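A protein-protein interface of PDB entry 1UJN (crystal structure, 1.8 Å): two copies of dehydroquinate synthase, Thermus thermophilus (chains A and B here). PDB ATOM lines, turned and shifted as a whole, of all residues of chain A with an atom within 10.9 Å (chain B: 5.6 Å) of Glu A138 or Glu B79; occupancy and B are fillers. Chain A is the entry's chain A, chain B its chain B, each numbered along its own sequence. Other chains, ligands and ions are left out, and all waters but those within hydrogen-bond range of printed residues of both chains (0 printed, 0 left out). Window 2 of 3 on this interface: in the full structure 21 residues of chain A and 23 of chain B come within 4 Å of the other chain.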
ATOM      1  N   LYS A  65      17.221 -13.120 -13.126  1.00  0.00           N
ATOM      2  CA  LYS A  65      15.797 -12.933 -13.377  1.00  0.00           C
ATOM      3  C   LYS A  65      14.970 -13.557 -12.261  1.00  0.00           C
ATOM      4  O   LYS A  65      14.236 -14.524 -12.475  1.00  0.00           O
ATOM      5  CB  LYS A  65      15.428 -13.531 -14.740  1.00  0.00           C
ATOM      6  CG  LYS A  65      16.020 -12.751 -15.906  1.00  0.00           C
ATOM      7  CD  LYS A  65      15.822 -13.444 -17.252  1.00  0.00           C
ATOM      8  CE  LYS A  65      14.354 -13.695 -17.573  1.00  0.00           C
ATOM      9  NZ  LYS A  65      14.208 -14.252 -18.955  1.00  0.00           N
ATOM     10  N   SER A  66      15.085 -12.977 -11.071  1.00  0.00           N
ATOM     11  CA  SER A  66      14.379 -13.470  -9.897  1.00  0.00           C
ATOM     12  C   SER A  66      13.771 -12.327  -9.096  1.00  0.00           C
ATOM     13  O   SER A  66      14.175 -11.174  -9.238  1.00  0.00           O
ATOM     14  CB  SER A  66      15.342 -14.234  -8.993  1.00  0.00           C
ATOM     15  OG  SER A  66      16.257 -13.339  -8.387  1.00  0.00           O
ATOM     16  N   LEU A  67      12.816 -12.662  -8.235  1.00  0.00           N
ATOM     17  CA  LEU A  67      12.155 -11.668  -7.397  1.00  0.00           C
ATOM     18  C   LEU A  67      13.152 -11.031  -6.440  1.00  0.00           C
ATOM     19  O   LEU A  67      13.056  -9.847  -6.123  1.00  0.00           O
ATOM     20  CB  LEU A  67      11.019 -12.315  -6.598  1.00  0.00           C
ATOM     21  CG  LEU A  67       9.736 -12.658  -7.361  1.00  0.00           C
ATOM     22  CD1 LEU A  67       8.879 -13.621  -6.546  1.00  0.00           C
ATOM     23  CD2 LEU A  67       8.976 -11.375  -7.662  1.00  0.00           C
ATOM     24  N   ILE A 134      10.860 -11.496 -15.287  1.00  0.00           N
ATOM     25  CA  ILE A 134      11.673 -12.379 -14.468  1.00  0.00           C
ATOM     26  C   ILE A 134      10.993 -13.746 -14.351  1.00  0.00           C
ATOM     27  O   ILE A 134       9.885 -13.947 -14.861  1.00  0.00           O
ATOM     28  CB  ILE A 134      11.869 -11.781 -13.055  1.00  0.00           C
ATOM     29  CG1 ILE A 134      10.505 -11.512 -12.410  1.00  0.00           C
ATOM     30  CG2 ILE A 134      12.666 -10.473 -13.144  1.00  0.00           C
ATOM     31  CD1 ILE A 134      10.579 -11.090 -10.951  1.00  0.00           C
ATOM     32  N   ASN A 135      11.659 -14.679 -13.674  1.00  0.00           N
ATOM     33  CA  ASN A 135      11.126 -16.025 -13.492  1.00  0.00           C
ATOM     34  C   ASN A 135      10.557 -16.210 -12.089  1.00  0.00           C
ATOM     35  O   ASN A 135      10.784 -15.391 -11.197  1.00  0.00           O
ATOM     36  CB  ASN A 135      12.225 -17.082 -13.684  1.00  0.00           C
ATOM     37  CG  ASN A 135      12.985 -16.916 -14.982  1.00  0.00           C
ATOM     38  OD1 ASN A 135      12.391 -16.746 -16.045  1.00  0.00           O
ATOM     39  ND2 ASN A 135      14.313 -16.983 -14.903  1.00  0.00           N
ATOM     40  N   LEU A 136       9.821 -17.304 -11.917  1.00  0.00           N
ATOM     41  CA  LEU A 136       9.241 -17.688 -10.633  1.00  0.00           C
ATOM     42  C   LEU A 136       9.588 -19.164 -10.473  1.00  0.00           C
ATOM     43  O   LEU A 136       9.926 -19.835 -11.447  1.00  0.00           O
ATOM     44  CB  LEU A 136       7.714 -17.553 -10.642  1.00  0.00           C
ATOM     45  CG  LEU A 136       7.072 -16.171 -10.742  1.00  0.00           C
ATOM     46  CD1 LEU A 136       5.556 -16.322 -10.869  1.00  0.00           C
ATOM     47  CD2 LEU A 136       7.432 -15.355  -9.519  1.00  0.00           C
ATOM     48  N   PRO A 137       9.517 -19.688  -9.243  1.00  0.00           N
ATOM     49  CA  PRO A 137       9.830 -21.106  -9.037  1.00  0.00           C
ATOM     50  C   PRO A 137       8.907 -21.970  -9.895  1.00  0.00           C
ATOM     51  O   PRO A 137       9.290 -23.050 -10.351  1.00  0.00           O
ATOM     52  CB  PRO A 137       9.572 -21.294  -7.548  1.00  0.00           C
ATOM     53  CG  PRO A 137       9.988 -19.976  -6.980  1.00  0.00           C
ATOM     54  CD  PRO A 137       9.372 -18.988  -7.954  1.00  0.00           C
ATOM     55  N   GLU A 138       7.691 -21.476 -10.118  1.00  0.00           N
ATOM     56  CA  GLU A 138       6.696 -22.186 -10.911  1.00  0.00           C
ATOM     57  C   GLU A 138       6.974 -22.170 -12.412  1.00  0.00           C
ATOM     58  O   GLU A 138       6.335 -22.901 -13.169  1.00  0.00           O
ATOM     59  CB  GLU A 138       5.301 -21.605 -10.664  1.00  0.00           C
ATOM     60  CG  GLU A 138       4.744 -21.791  -9.251  1.00  0.00           C
ATOM     61  CD  GLU A 138       5.491 -20.991  -8.199  1.00  0.00           C
ATOM     62  OE1 GLU A 138       6.076 -19.945  -8.543  1.00  0.00           O
ATOM     63  OE2 GLU A 138       5.477 -21.398  -7.017  1.00  0.00           O
ATOM     64  N   GLY A 139       7.907 -21.334 -12.856  1.00  0.00           N
ATOM     65  CA  GLY A 139       8.193 -21.301 -14.278  1.00  0.00           C
ATOM     66  C   GLY A 139       8.937 -20.084 -14.782  1.00  0.00           C
ATOM     67  O   GLY A 139       8.979 -19.045 -14.127  1.00  0.00           O
ATOM     68  N   LYS A 140       9.520 -20.222 -15.967  1.00  0.00           N
ATOM     69  CA  LYS A 140      10.277 -19.147 -16.590  1.00  0.00           C
ATOM     70  C   LYS A 140       9.360 -18.064 -17.144  1.00  0.00           C
ATOM     71  O   LYS A 140       8.264 -18.351 -17.619  1.00  0.00           O
ATOM     72  CB  LYS A 140      11.117 -19.690 -17.749  1.00  0.00           C
ATOM     73  CG  LYS A 140      12.157 -20.729 -17.366  1.00  0.00           C
ATOM     74  CD  LYS A 140      13.288 -20.113 -16.574  1.00  0.00           C
ATOM     75  CE  LYS A 140      14.411 -21.121 -16.372  1.00  0.00           C
ATOM     76  NZ  LYS A 140      15.550 -20.556 -15.600  1.00  0.00           N
ATOM     77  N   ASN A 141       9.829 -16.823 -17.072  1.00  0.00           N
ATOM     78  CA  ASN A 141       9.112 -15.670 -17.615  1.00  0.00           C
ATOM     79  C   ASN A 141       7.612 -15.611 -17.335  1.00  0.00           C
ATOM     80  O   ASN A 141       6.808 -15.504 -18.265  1.00  0.00           O
ATOM     81  CB  ASN A 141       9.338 -15.623 -19.124  1.00  0.00           C
ATOM     82  CG  ASN A 141      10.807 -15.646 -19.494  1.00  0.00           C
ATOM     83  OD1 ASN A 141      11.573 -14.784 -19.068  1.00  0.00           O
ATOM     84  ND2 ASN A 141      11.210 -16.637 -20.290  1.00  0.00           N
ATOM     85  N   LEU A 142       7.230 -15.654 -16.064  1.00  0.00           N
ATOM     86  CA  LEU A 142       5.817 -15.604 -15.718  1.00  0.00           C
ATOM     87  C   LEU A 142       5.393 -14.248 -15.166  1.00  0.00           C
ATOM     88  O   LEU A 142       4.210 -14.012 -14.933  1.00  0.00           O
ATOM     89  CB  LEU A 142       5.487 -16.704 -14.708  1.00  0.00           C
ATOM     90  CG  LEU A 142       5.678 -18.134 -15.224  1.00  0.00           C
ATOM     91  CD1 LEU A 142       5.368 -19.123 -14.111  1.00  0.00           C
ATOM     92  CD2 LEU A 142       4.771 -18.376 -16.413  1.00  0.00           C
ATOM     93  N   VAL A 143       6.363 -13.365 -14.955  1.00  0.00           N
ATOM     94  CA  VAL A 143       6.094 -12.028 -14.431  1.00  0.00           C
ATOM     95  C   VAL A 143       6.883 -11.044 -15.273  1.00  0.00           C
ATOM     96  O   VAL A 143       8.062 -11.256 -15.547  1.00  0.00           O
ATOM     97  CB  VAL A 143       6.539 -11.894 -12.959  1.00  0.00           C
ATOM     98  CG1 VAL A 143       6.140 -10.518 -12.410  1.00  0.00           C
ATOM     99  CG2 VAL A 143       5.901 -13.007 -12.123  1.00  0.00           C
ATOM    100  N   HIS A 235      11.135 -25.452 -26.741  1.00  0.00           N
ATOM    101  CA  HIS A 235      10.691 -25.247 -25.373  1.00  0.00           C
ATOM    102  C   HIS A 235      10.630 -26.574 -24.620  1.00  0.00           C
ATOM    103  O   HIS A 235      11.029 -26.660 -23.457  1.00  0.00           O
ATOM    104  CB  HIS A 235       9.309 -24.600 -25.374  1.00  0.00           C
ATOM    105  CG  HIS A 235       8.747 -24.382 -24.007  1.00  0.00           C
ATOM    106  ND1 HIS A 235       9.195 -23.384 -23.170  1.00  0.00           N
ATOM    107  CD2 HIS A 235       7.784 -25.044 -23.325  1.00  0.00           C
ATOM    108  CE1 HIS A 235       8.530 -23.440 -22.028  1.00  0.00           C
ATOM    109  NE2 HIS A 235       7.668 -24.437 -22.097  1.00  0.00           N
ATOM    110  N   ALA A 239      12.854 -27.730 -21.324  1.00  0.00           N
ATOM    111  CA  ALA A 239      12.190 -28.188 -20.110  1.00  0.00           C
ATOM    112  C   ALA A 239      12.680 -29.566 -19.676  1.00  0.00           C
ATOM    113  O   ALA A 239      12.943 -29.800 -18.492  1.00  0.00           O
ATOM    114  CB  ALA A 239      10.677 -28.212 -20.321  1.00  0.00           C
ATOM    115  N   ARG A 242      15.987 -29.688 -17.994  1.00  0.00           N
ATOM    116  CA  ARG A 242      16.031 -28.872 -16.789  1.00  0.00           C
ATOM    117  C   ARG A 242      16.722 -27.555 -17.094  1.00  0.00           C
ATOM    118  O   ARG A 242      17.360 -26.954 -16.227  1.00  0.00           O
ATOM    119  CB  ARG A 242      16.768 -29.606 -15.670  1.00  0.00           C
ATOM    120  CG  ARG A 242      15.868 -30.452 -14.793  1.00  0.00           C
ATOM    121  CD  ARG A 242      15.022 -31.420 -15.600  1.00  0.00           C
ATOM    122  NE  ARG A 242      13.895 -31.916 -14.815  1.00  0.00           N
ATOM    123  CZ  ARG A 242      12.972 -31.138 -14.257  1.00  0.00           C
ATOM    124  NH1 ARG A 242      13.034 -29.818 -14.397  1.00  0.00           N
ATOM    125  NH2 ARG A 242      11.981 -31.675 -13.555  1.00  0.00           N
ATOM    126  N   HIS A 243      16.603 -27.132 -18.348  1.00  0.00           N
ATOM    127  CA  HIS A 243      17.171 -25.882 -18.822  1.00  0.00           C
ATOM    128  C   HIS A 243      18.686 -25.865 -18.957  1.00  0.00           C
ATOM    129  O   HIS A 243      19.299 -24.800 -19.042  1.00  0.00           O
ATOM    130  CB  HIS A 243      16.676 -24.747 -17.928  1.00  0.00           C
ATOM    131  CG  HIS A 243      15.184 -24.657 -17.874  1.00  0.00           C
ATOM    132  ND1 HIS A 243      14.454 -25.090 -16.789  1.00  0.00           N
ATOM    133  CD2 HIS A 243      14.295 -24.089 -18.723  1.00  0.00           C
ATOM    134  CE1 HIS A 243      13.180 -24.789 -16.969  1.00  0.00           C
ATOM    135  NE2 HIS A 243      13.057 -24.179 -18.135  1.00  0.00           N
ATOM    136  N   LEU B  74       1.806 -13.964  -6.891  1.00  0.00           N
ATOM    137  CA  LEU B  74       2.184 -14.380  -8.242  1.00  0.00           C
ATOM    138  C   LEU B  74       2.427 -15.891  -8.337  1.00  0.00           C
ATOM    139  O   LEU B  74       1.983 -16.545  -9.288  1.00  0.00           O
ATOM    140  CB  LEU B  74       3.435 -13.624  -8.702  1.00  0.00           C
ATOM    141  CG  LEU B  74       3.250 -12.124  -8.972  1.00  0.00           C
ATOM    142  CD1 LEU B  74       4.603 -11.447  -9.005  1.00  0.00           C
ATOM    143  CD2 LEU B  74       2.508 -11.915 -10.288  1.00  0.00           C
ATOM    144  N   SER B  75       3.130 -16.458  -7.365  1.00  0.00           N
ATOM    145  CA  SER B  75       3.387 -17.896  -7.403  1.00  0.00           C
ATOM    146  C   SER B  75       2.103 -18.690  -7.201  1.00  0.00           C
ATOM    147  O   SER B  75       1.944 -19.778  -7.761  1.00  0.00           O
ATOM    148  CB  SER B  75       4.432 -18.285  -6.355  1.00  0.00           C
ATOM    149  OG  SER B  75       5.721 -17.857  -6.766  1.00  0.00           O
ATOM    150  N   TRP B  76       1.184 -18.134  -6.415  1.00  0.00           N
ATOM    151  CA  TRP B  76      -0.100 -18.774  -6.153  1.00  0.00           C
ATOM    152  C   TRP B  76      -0.909 -18.844  -7.453  1.00  0.00           C
ATOM    153  O   TRP B  76      -1.556 -19.852  -7.740  1.00  0.00           O
ATOM    154  CB  TRP B  76      -0.869 -17.986  -5.092  1.00  0.00           C
ATOM    155  CG  TRP B  76      -2.229 -18.542  -4.787  1.00  0.00           C
ATOM    156  CD1 TRP B  76      -2.517 -19.656  -4.045  1.00  0.00           C
ATOM    157  CD2 TRP B  76      -3.484 -18.021  -5.237  1.00  0.00           C
ATOM    158  NE1 TRP B  76      -3.879 -19.859  -4.006  1.00  0.00           N
ATOM    159  CE2 TRP B  76      -4.496 -18.870  -4.729  1.00  0.00           C
ATOM    160  CE3 TRP B  76      -3.854 -16.921  -6.020  1.00  0.00           C
ATOM    161  CZ2 TRP B  76      -5.854 -18.650  -4.980  1.00  0.00           C
ATOM    162  CZ3 TRP B  76      -5.207 -16.702  -6.271  1.00  0.00           C
ATOM    163  CH2 TRP B  76      -6.191 -17.565  -5.751  1.00  0.00           C
ATOM    164  N   LEU B  77      -0.873 -17.767  -8.238  1.00  0.00           N
ATOM    165  CA  LEU B  77      -1.580 -17.741  -9.515  1.00  0.00           C
ATOM    166  C   LEU B  77      -0.939 -18.731 -10.479  1.00  0.00           C
ATOM    167  O   LEU B  77      -1.633 -19.483 -11.160  1.00  0.00           O
ATOM    168  CB  LEU B  77      -1.534 -16.336 -10.138  1.00  0.00           C
ATOM    169  CG  LEU B  77      -2.281 -15.233  -9.386  1.00  0.00           C
ATOM    170  CD1 LEU B  77      -2.069 -13.900 -10.090  1.00  0.00           C
ATOM    171  CD2 LEU B  77      -3.762 -15.566  -9.319  1.00  0.00           C
ATOM    172  N   ALA B  78       0.388 -18.723 -10.536  1.00  0.00           N
ATOM    173  CA  ALA B  78       1.118 -19.616 -11.428  1.00  0.00           C
ATOM    174  C   ALA B  78       0.846 -21.061 -11.023  1.00  0.00           C
ATOM    175  O   ALA B  78       0.674 -21.945 -11.861  1.00  0.00           O
ATOM    176  CB  ALA B  78       2.607 -19.319 -11.350  1.00  0.00           C
ATOM    177  N   GLU B  79       0.810 -21.276  -9.717  1.00  0.00           N
ATOM    178  CA  GLU B  79       0.551 -22.581  -9.131  1.00  0.00           C
ATOM    179  C   GLU B  79      -0.775 -23.125  -9.674  1.00  0.00           C
ATOM    180  O   GLU B  79      -0.884 -24.299 -10.030  1.00  0.00           O
ATOM    181  CB  GLU B  79       0.489 -22.406  -7.614  1.00  0.00           C
ATOM    182  CG  GLU B  79       0.626 -23.648  -6.764  1.00  0.00           C
ATOM    183  CD  GLU B  79       0.980 -23.279  -5.332  1.00  0.00           C
ATOM    184  OE1 GLU B  79       2.150 -22.902  -5.088  1.00  0.00           O
ATOM    185  OE2 GLU B  79       0.089 -23.344  -4.454  1.00  0.00           O
ATOM    186  N   LYS B  80      -1.780 -22.259  -9.739  1.00  0.00           N
ATOM    187  CA  LYS B  80      -3.089 -22.657 -10.229  1.00  0.00           C
ATOM    188  C   LYS B  80      -3.114 -22.693 -11.755  1.00  0.00           C
ATOM    189  O   LYS B  80      -4.069 -23.139 -12.376  1.00  0.00           O
ATOM    190  CB  LYS B  80      -4.119 -21.652  -9.714  1.00  0.00           C
ATOM    191  CG  LYS B  80      -4.852 -22.156  -8.469  1.00  0.00           C
ATOM    192  CD  LYS B  80      -4.002 -22.027  -7.204  1.00  0.00           C
ATOM    193  CE  LYS B  80      -4.826 -22.207  -5.924  1.00  0.00           C
ATOM    194  NZ  LYS B  80      -4.118 -23.094  -5.003  1.00  0.00           N
ATOM    195  N   GLY B  81      -2.036 -22.221 -12.372  1.00  0.00           N
ATOM    196  CA  GLY B  81      -1.949 -22.232 -13.820  1.00  0.00           C
ATOM    197  C   GLY B  81      -2.895 -21.287 -14.543  1.00  0.00           C
ATOM    198  O   GLY B  81      -3.394 -21.610 -15.621  1.00  0.00           O
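Hydrophobic or aromatic side chains of chain A within 4 Å of the printed part of chain B: Leu A136, Leu A142 and Val A143.
Of the printed residues of chain B, Glu A138 touches Ser B75 (2.8 Å), Ala B78 (3.6 Å) and Glu B79 (3.99 Å).
Printed residues of chain A within 4 Å of Glu B79: Glu A138.
Ala B78 touches two residues of chain A.
No residue of chain A comes within 4 Å of Gly B81.
Printed residues of chain A within 4 Å of Leu B74: Leu A136 (3.9 Å) and Val A143 (3.7 Å).
Of the printed residues of chain A, Ser B75 touches Glu A138 (2.8 Å).
Asn A141 touches none of the printed residues of chain B.
The nearest printed residue of chain B that does not touch Glu A138 is Leu B74 (5.4 Å).
The nearest printed residue of chain A that does not touch Glu B79 is Leu A142 (6.7 Å).
The nearest printed residue of chain B that does not touch Leu A136 is Ser B75 (4.1 Å).
No position is printed for both chains.
Of the 6 pairs that touch across the chains among the printed residues, none has its exchanged pair printed and touching as well.
The side-chain hydroxyl (OG) of Ser B75 is in hydrogen-bond range of the side-chain carboxylate (OE1) of Glu A138 (2.8 Å).
N of Leu A142 sits at hydrogen-bond distance from O of Ile A134.
The backbone NH of Ile A134 sits at hydrogen-bond distance from the backbone carbonyl oxygen of Val A143 (2.8 Å).
Leu B74 touches Leu A136.
Glu A138 touches Ala B78.
Glu A138 touches Glu B79 (CG to N, 3.99 Å).
Ala B78 touches Leu A142 (CB to CD1, 3.9 Å).
Val A143 touches Leu B74 (CG2 to CD1, 3.7 Å).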
